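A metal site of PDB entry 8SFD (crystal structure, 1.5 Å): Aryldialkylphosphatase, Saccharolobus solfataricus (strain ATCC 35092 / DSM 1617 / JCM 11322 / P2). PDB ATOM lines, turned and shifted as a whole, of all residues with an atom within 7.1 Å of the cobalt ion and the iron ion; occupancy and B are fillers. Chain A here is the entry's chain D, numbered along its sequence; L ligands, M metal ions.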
ATOM      1  N   HIS A  22       0.183  -4.719  -0.544  1.00  0.00           N
ATOM      2  CA  HIS A  22      -0.129  -3.471  -1.235  1.00  0.00           C
ATOM      3  C   HIS A  22       0.526  -3.442  -2.617  1.00  0.00           C
ATOM      4  O   HIS A  22       1.668  -2.995  -2.764  1.00  0.00           O
ATOM      5  CB  HIS A  22       0.295  -2.253  -0.399  1.00  0.00           C
ATOM      6  CG  HIS A  22      -0.204  -0.929  -0.889  1.00  0.00           C
ATOM      7  ND1 HIS A  22      -0.682   0.039  -0.034  1.00  0.00           N
ATOM      8  CD2 HIS A  22      -0.295  -0.395  -2.128  1.00  0.00           C
ATOM      9  CE1 HIS A  22      -1.046   1.106  -0.725  1.00  0.00           C
ATOM     10  NE2 HIS A  22      -0.818   0.865  -1.999  1.00  0.00           N
ATOM     11  N   GLU A  23      -0.218  -3.912  -3.621  1.00  0.00           N
ATOM     12  CA  GLU A  23       0.201  -3.870  -5.019  1.00  0.00           C
ATOM     13  C   GLU A  23      -0.990  -3.479  -5.884  1.00  0.00           C
ATOM     14  O   GLU A  23      -2.135  -3.718  -5.502  1.00  0.00           O
ATOM     15  CB  GLU A  23       0.744  -5.232  -5.456  1.00  0.00           C
ATOM     16  CG  GLU A  23       1.766  -5.838  -4.513  1.00  0.00           C
ATOM     17  CD  GLU A  23       3.090  -5.094  -4.457  1.00  0.00           C
ATOM     18  OE1 GLU A  23       3.872  -5.366  -3.520  1.00  0.00           O
ATOM     19  OE2 GLU A  23       3.344  -4.269  -5.357  1.00  0.00           O
ATOM     20  N   HIS A  24      -0.715  -2.894  -7.059  1.00  0.00           N
ATOM     21  CA  HIS A  24      -1.773  -2.504  -7.982  1.00  0.00           C
ATOM     22  C   HIS A  24      -1.587  -3.211  -9.316  1.00  0.00           C
ATOM     23  O   HIS A  24      -0.581  -3.013  -9.991  1.00  0.00           O
ATOM     24  CB  HIS A  24      -1.755  -0.995  -8.223  1.00  0.00           C
ATOM     25  CG  HIS A  24      -1.959  -0.164  -7.000  1.00  0.00           C
ATOM     26  ND1 HIS A  24      -3.205   0.228  -6.545  1.00  0.00           N
ATOM     27  CD2 HIS A  24      -1.078   0.381  -6.151  1.00  0.00           C
ATOM     28  CE1 HIS A  24      -3.057   0.957  -5.450  1.00  0.00           C
ATOM     29  NE2 HIS A  24      -1.781   1.064  -5.184  1.00  0.00           N
ATOM     30  N   PRO A  67      -5.119  -2.528  -3.270  1.00  0.00           N
ATOM     31  CA  PRO A  67      -5.939  -1.445  -2.733  1.00  0.00           C
ATOM     32  C   PRO A  67      -6.294  -0.340  -3.730  1.00  0.00           C
ATOM     33  O   PRO A  67      -6.316   0.838  -3.384  1.00  0.00           O
ATOM     34  CB  PRO A  67      -5.051  -0.901  -1.598  1.00  0.00           C
ATOM     35  CG  PRO A  67      -3.633  -1.140  -2.070  1.00  0.00           C
ATOM     36  CD  PRO A  67      -3.688  -2.348  -2.980  1.00  0.00           C
ATOM     37  N   THR A  68      -6.578  -0.753  -4.970  1.00  0.00           N
ATOM     38  CA  THR A  68      -7.099   0.140  -5.998  1.00  0.00           C
ATOM     39  C   THR A  68      -8.590   0.359  -5.747  1.00  0.00           C
ATOM     40  O   THR A  68      -9.353  -0.602  -5.792  1.00  0.00           O
ATOM     41  CB  THR A  68      -6.886  -0.441  -7.402  1.00  0.00           C
ATOM     42  OG1 THR A  68      -5.522  -0.856  -7.574  1.00  0.00           O
ATOM     43  CG2 THR A  68      -7.250   0.549  -8.489  1.00  0.00           C
ATOM     44  N   PHE A  97     -10.342   7.194  -2.708  1.00  0.00           N
ATOM     45  CA  PHE A  97      -8.996   7.750  -2.719  1.00  0.00           C
ATOM     46  C   PHE A  97      -9.067   9.207  -3.147  1.00  0.00           C
ATOM     47  O   PHE A  97      -9.185   9.500  -4.342  1.00  0.00           O
ATOM     48  CB  PHE A  97      -8.109   6.896  -3.629  1.00  0.00           C
ATOM     49  CG  PHE A  97      -6.637   7.180  -3.543  1.00  0.00           C
ATOM     50  CD1 PHE A  97      -6.072   8.270  -4.207  1.00  0.00           C
ATOM     51  CD2 PHE A  97      -5.809   6.370  -2.796  1.00  0.00           C
ATOM     52  CE1 PHE A  97      -4.716   8.522  -4.117  1.00  0.00           C
ATOM     53  CE2 PHE A  97      -4.446   6.635  -2.708  1.00  0.00           C
ATOM     54  CZ  PHE A  97      -3.912   7.708  -3.368  1.00  0.00           C
ATOM     55  N   PHE A  99      -7.501  13.387  -1.934  1.00  0.00           N
ATOM     56  CA  PHE A  99      -6.591  14.181  -1.122  1.00  0.00           C
ATOM     57  C   PHE A  99      -7.257  15.473  -0.647  1.00  0.00           C
ATOM     58  O   PHE A  99      -6.794  16.050   0.337  1.00  0.00           O
ATOM     59  CB  PHE A  99      -5.328  14.524  -1.906  1.00  0.00           C
ATOM     60  CG  PHE A  99      -4.409  13.373  -2.196  1.00  0.00           C
ATOM     61  CD1 PHE A  99      -4.618  12.120  -1.637  1.00  0.00           C
ATOM     62  CD2 PHE A  99      -3.319  13.534  -3.043  1.00  0.00           C
ATOM     63  CE1 PHE A  99      -3.768  11.059  -1.914  1.00  0.00           C
ATOM     64  CE2 PHE A  99      -2.469  12.474  -3.320  1.00  0.00           C
ATOM     65  CZ  PHE A  99      -2.690  11.242  -2.764  1.00  0.00           C
ATOM     66  N   KCX A 137     -10.002   0.970   1.892  1.00  0.00           N
ATOM     67  CA  KCX A 137      -8.832   1.827   1.577  1.00  0.00           C
ATOM     68  CB  KCX A 137      -8.303   1.517   0.180  1.00  0.00           C
ATOM     69  CG  KCX A 137      -7.225   2.478  -0.331  1.00  0.00           C
ATOM     70  CD  KCX A 137      -5.927   2.384   0.442  1.00  0.00           C
ATOM     71  CE  KCX A 137      -4.843   3.289  -0.104  1.00  0.00           C
ATOM     72  NZ  KCX A 137      -4.370   2.885  -1.420  1.00  0.00           N
ATOM     73  C   KCX A 137      -9.233   3.297   1.696  1.00  0.00           C
ATOM     74  O   KCX A 137     -10.266   3.676   1.109  1.00  0.00           O
ATOM     75  CX  KCX A 137      -3.178   3.293  -1.887  1.00  0.00           C
ATOM     76  OQ1 KCX A 137      -2.933   2.830  -3.115  1.00  0.00           O
ATOM     77  OQ2 KCX A 137      -2.410   3.994  -1.268  1.00  0.00           O
ATOM     78  N   ILE A 138      -8.415   4.082   2.436  1.00  0.00           N
ATOM     79  CA  ILE A 138      -8.606   5.555   2.599  1.00  0.00           C
ATOM     80  C   ILE A 138      -7.262   6.242   2.377  1.00  0.00           C
ATOM     81  O   ILE A 138      -6.224   5.584   2.424  1.00  0.00           O
ATOM     82  CB  ILE A 138      -9.205   5.880   3.984  1.00  0.00           C
ATOM     83  CG1 ILE A 138      -8.234   5.520   5.109  1.00  0.00           C
ATOM     84  CG2 ILE A 138     -10.563   5.208   4.162  1.00  0.00           C
ATOM     85  CD1 ILE A 138      -8.730   5.876   6.497  1.00  0.00           C
ATOM     86  N   ALA A 139      -7.302   7.558   2.139  1.00  0.00           N
ATOM     87  CA  ALA A 139      -6.094   8.308   1.815  1.00  0.00           C
ATOM     88  C   ALA A 139      -6.116   9.701   2.438  1.00  0.00           C
ATOM     89  O   ALA A 139      -7.166  10.267   2.698  1.00  0.00           O
ATOM     90  CB  ALA A 139      -5.937   8.402   0.317  1.00  0.00           C
ATOM     91  N   ASP A 141      -2.892  13.149   2.126  1.00  0.00           N
ATOM     92  CA  ASP A 141      -1.557  13.462   1.643  1.00  0.00           C
ATOM     93  C   ASP A 141      -1.208  14.887   2.046  1.00  0.00           C
ATOM     94  O   ASP A 141      -1.564  15.323   3.135  1.00  0.00           O
ATOM     95  CB  ASP A 141      -1.460  13.195   0.137  1.00  0.00           C
ATOM     96  CG  ASP A 141      -0.053  12.911  -0.357  1.00  0.00           C
ATOM     97  OD1 ASP A 141       0.697  13.885  -0.593  1.00  0.00           O
ATOM     98  OD2 ASP A 141       0.292  11.719  -0.485  1.00  0.00           O
ATOM     99  N   THR A 169      -4.412   2.319   4.719  1.00  0.00           N
ATOM    100  CA  THR A 169      -4.372   3.733   4.398  1.00  0.00           C
ATOM    101  C   THR A 169      -3.197   4.072   3.484  1.00  0.00           C
ATOM    102  O   THR A 169      -2.194   3.363   3.412  1.00  0.00           O
ATOM    103  CB  THR A 169      -4.308   4.639   5.645  1.00  0.00           C
ATOM    104  OG1 THR A 169      -2.941   4.848   6.019  1.00  0.00           O
ATOM    105  CG2 THR A 169      -5.106   4.093   6.802  1.00  0.00           C
ATOM    106  N   HIS A 170      -3.404   5.168   2.751  1.00  0.00           N
ATOM    107  CA  HIS A 170      -2.350   5.937   2.119  1.00  0.00           C
ATOM    108  C   HIS A 170      -2.113   7.179   2.985  1.00  0.00           C
ATOM    109  O   HIS A 170      -3.076   7.840   3.348  1.00  0.00           O
ATOM    110  CB  HIS A 170      -2.814   6.358   0.712  1.00  0.00           C
ATOM    111  CG  HIS A 170      -1.978   7.391   0.047  1.00  0.00           C
ATOM    112  ND1 HIS A 170      -1.230   7.103  -1.079  1.00  0.00           N
ATOM    113  CD2 HIS A 170      -1.756   8.685   0.312  1.00  0.00           C
ATOM    114  CE1 HIS A 170      -0.592   8.190  -1.475  1.00  0.00           C
ATOM    115  NE2 HIS A 170      -0.900   9.168  -0.646  1.00  0.00           N
ATOM    116  N   SER A 171      -0.850   7.447   3.328  1.00  0.00           N
ATOM    117  CA  SER A 171      -0.500   8.670   4.033  1.00  0.00           C
ATOM    118  C   SER A 171       0.719   9.320   3.386  1.00  0.00           C
ATOM    119  O   SER A 171       1.388   8.708   2.554  1.00  0.00           O
ATOM    120  CB  SER A 171      -0.286   8.423   5.523  1.00  0.00           C
ATOM    121  OG  SER A 171       1.023   7.945   5.799  1.00  0.00           O
ATOM    122  N   GLY A 198      -0.166   3.460   5.817  1.00  0.00           N
ATOM    123  CA  GLY A 198       0.629   3.248   4.619  1.00  0.00           C
ATOM    124  C   GLY A 198       1.698   4.314   4.373  1.00  0.00           C
ATOM    125  O   GLY A 198       1.573   5.462   4.801  1.00  0.00           O
ATOM    126  N   HIS A 199       2.757   3.875   3.679  1.00  0.00           N
ATOM    127  CA  HIS A 199       3.746   4.739   3.051  1.00  0.00           C
ATOM    128  C   HIS A 199       4.710   5.323   4.075  1.00  0.00           C
ATOM    129  O   HIS A 199       5.370   6.319   3.813  1.00  0.00           O
ATOM    130  CB  HIS A 199       3.058   5.822   2.205  1.00  0.00           C
ATOM    131  CG  HIS A 199       2.159   5.258   1.153  1.00  0.00           C
ATOM    132  ND1 HIS A 199       2.301   3.980   0.656  1.00  0.00           N
ATOM    133  CD2 HIS A 199       1.130   5.805   0.491  1.00  0.00           C
ATOM    134  CE1 HIS A 199       1.355   3.764  -0.258  1.00  0.00           C
ATOM    135  NE2 HIS A 199       0.644   4.856  -0.373  1.00  0.00           N
ATOM    136  N   ASP A 222       6.157   0.135   2.219  1.00  0.00           N
ATOM    137  CA  ASP A 222       5.300  -0.479   1.221  1.00  0.00           C
ATOM    138  C   ASP A 222       5.493   0.116  -0.172  1.00  0.00           C
ATOM    139  O   ASP A 222       4.649  -0.118  -1.040  1.00  0.00           O
ATOM    140  CB  ASP A 222       3.837  -0.385   1.646  1.00  0.00           C
ATOM    141  CG  ASP A 222       3.355   1.035   1.942  1.00  0.00           C
ATOM    142  OD1 ASP A 222       4.028   1.984   1.492  1.00  0.00           O
ATOM    143  OD2 ASP A 222       2.317   1.167   2.615  1.00  0.00           O
ATOM    144  N   ARG A 223       6.605   0.827  -0.427  1.00  0.00           N
ATOM    145  CA  ARG A 223       6.783   1.461  -1.725  1.00  0.00           C
ATOM    146  C   ARG A 223       8.154   1.122  -2.316  1.00  0.00           C
ATOM    147  O   ARG A 223       8.781   1.946  -2.974  1.00  0.00           O
ATOM    148  CB  ARG A 223       6.578   2.973  -1.602  1.00  0.00           C
ATOM    149  CG  ARG A 223       5.114   3.385  -1.674  1.00  0.00           C
ATOM    150  CD  ARG A 223       4.903   4.885  -1.549  1.00  0.00           C
ATOM    151  NE  ARG A 223       3.746   5.325  -2.309  1.00  0.00           N
ATOM    152  CZ  ARG A 223       3.273   6.571  -2.310  1.00  0.00           C
ATOM    153  NH1 ARG A 223       3.819   7.483  -1.537  1.00  0.00           N
ATOM    154  NH2 ARG A 223       2.253   6.880  -3.088  1.00  0.00           N
ATOM    155  N   LEU A 226       8.469   1.768  -6.186  1.00  0.00           N
ATOM    156  CA  LEU A 226       8.406   3.124  -6.714  1.00  0.00           C
ATOM    157  C   LEU A 226       9.730   3.825  -6.451  1.00  0.00           C
ATOM    158  O   LEU A 226      10.358   3.604  -5.419  1.00  0.00           O
ATOM    159  CB  LEU A 226       7.253   3.880  -6.053  1.00  0.00           C
ATOM    160  CG  LEU A 226       5.853   3.278  -6.226  1.00  0.00           C
ATOM    161  CD1 LEU A 226       4.792   4.247  -5.730  1.00  0.00           C
ATOM    162  CD2 LEU A 226       5.596   2.896  -7.673  1.00  0.00           C
ATOM    163  N   ASP A 256       3.987  -1.426  -3.781  1.00  0.00           N
ATOM    164  CA  ASP A 256       3.093  -0.426  -4.337  1.00  0.00           C
ATOM    165  C   ASP A 256       3.383  -0.330  -5.829  1.00  0.00           C
ATOM    166  O   ASP A 256       3.247   0.730  -6.439  1.00  0.00           O
ATOM    167  CB  ASP A 256       3.260   0.923  -3.633  1.00  0.00           C
ATOM    168  CG  ASP A 256       2.087   1.880  -3.787  1.00  0.00           C
ATOM    169  OD1 ASP A 256       1.025   1.472  -4.294  1.00  0.00           O
ATOM    170  OD2 ASP A 256       2.245   3.041  -3.370  1.00  0.00           O
ATOM    171  N   TYR A 257       3.832  -1.451  -6.409  1.00  0.00           N
ATOM    172  CA  TYR A 257       4.141  -1.478  -7.827  1.00  0.00           C
ATOM    173  C   TYR A 257       2.832  -1.453  -8.611  1.00  0.00           C
ATOM    174  O   TYR A 257       1.908  -2.209  -8.324  1.00  0.00           O
ATOM    175  CB  TYR A 257       4.981  -2.701  -8.201  1.00  0.00           C
ATOM    176  CG  TYR A 257       5.456  -2.683  -9.635  1.00  0.00           C
ATOM    177  CD1 TYR A 257       6.378  -1.744 -10.062  1.00  0.00           C
ATOM    178  CD2 TYR A 257       4.939  -3.558 -10.573  1.00  0.00           C
ATOM    179  CE1 TYR A 257       6.802  -1.689 -11.377  1.00  0.00           C
ATOM    180  CE2 TYR A 257       5.354  -3.523 -11.891  1.00  0.00           C
ATOM    181  CZ  TYR A 257       6.293  -2.597 -12.296  1.00  0.00           C
ATOM    182  OH  TYR A 257       6.711  -2.554 -13.608  1.00  0.00           O
ATOM    183  N   CYS A 258       2.779  -0.552  -9.596  1.00  0.00           N
ATOM    184  CA  CYS A 258       1.669  -0.506 -10.538  1.00  0.00           C
ATOM    185  C   CYS A 258       2.114  -1.156 -11.838  1.00  0.00           C
ATOM    186  O   CYS A 258       2.988  -0.630 -12.539  1.00  0.00           O
ATOM    187  CB  CYS A 258       1.225   0.939 -10.771  1.00  0.00           C
ATOM    188  SG  CYS A 258       0.780   1.802  -9.244  1.00  0.00           S
HETATM  189  P1  LIG L   1      -0.450   4.763  -4.374  1.00  0.00           P
HETATM  190  O1  LIG L   1       0.922   5.130  -4.946  1.00  0.00           O
HETATM  191  O2  LIG L   1      -0.288   3.959  -3.079  1.00  0.00           O
HETATM  192  O3  LIG L   1      -1.207   3.915  -5.394  1.00  0.00           O
HETATM  193  O4  LIG L   1      -1.235   6.034  -4.074  1.00  0.00           O
HETATM  194 CO    CO M   1      -0.844   5.170  -1.768  1.00  0.00          CO
HETATM  195 FE    FE M   2      -0.988   2.184  -3.675  1.00  0.00          FE
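O of Pro 67 lies within hydrogen-bond range of NZ of KCX 137 (3.4 Å). The backbone NH of His 24 is in hydrogen-bond range of the backbone carbonyl oxygen of Tyr 257. ND1 of His 199 lies within hydrogen-bond range of OD1 of Asp 222, at 2.8 Å. The side-chain carboxylate (OD2) of Asp 141 is in hydrogen-bond range of a ring nitrogen (NE2) of His 170 (2.8 Å). The backbone carbonyl oxygen of Ile 138 lies within hydrogen-bond range of the backbone NH of His 170. The guanidinium group of Arg 223 is in salt-bridge range of the side-chain carboxylate of Asp 256, 2.9 Å away. OE2 of Glu 23 is in hydrogen-bond range of N of Asp 256, at 3.3 Å. O of Asp 222 lies within hydrogen-bond range of N of Asp 256 (3.1 Å).
Residues that only touch the cobalt ion: Arg 223. Four residues have an atom within 4 Å of the cobalt ion: KCX 137, His 170, His 199 and Arg 223. The nearest printed residue that does not touch the cobalt ion is Phe 97 (4.001 Å).
The nearest printed residue that does not touch the iron ion is His 199 (4.4 Å).
The cobalt ion is bound by an oxygen (O2) of the ligand (1.9 Å), OQ2 of KCX 137 (2.0 Å), a ring nitrogen (NE2) of His 199 (2.1 Å), a ring nitrogen (ND1) of His 170 (2.1 Å) and an oxygen (O4) of the ligand (2.5 Å). The cobalt ion has five donor atoms within binding distance.
The iron ion is bound by O2 of the ligand, NE2 of His 24, OQ1 of KCX 137, NE2 of His 22, OD1 of Asp 256 and O3 of the ligand.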
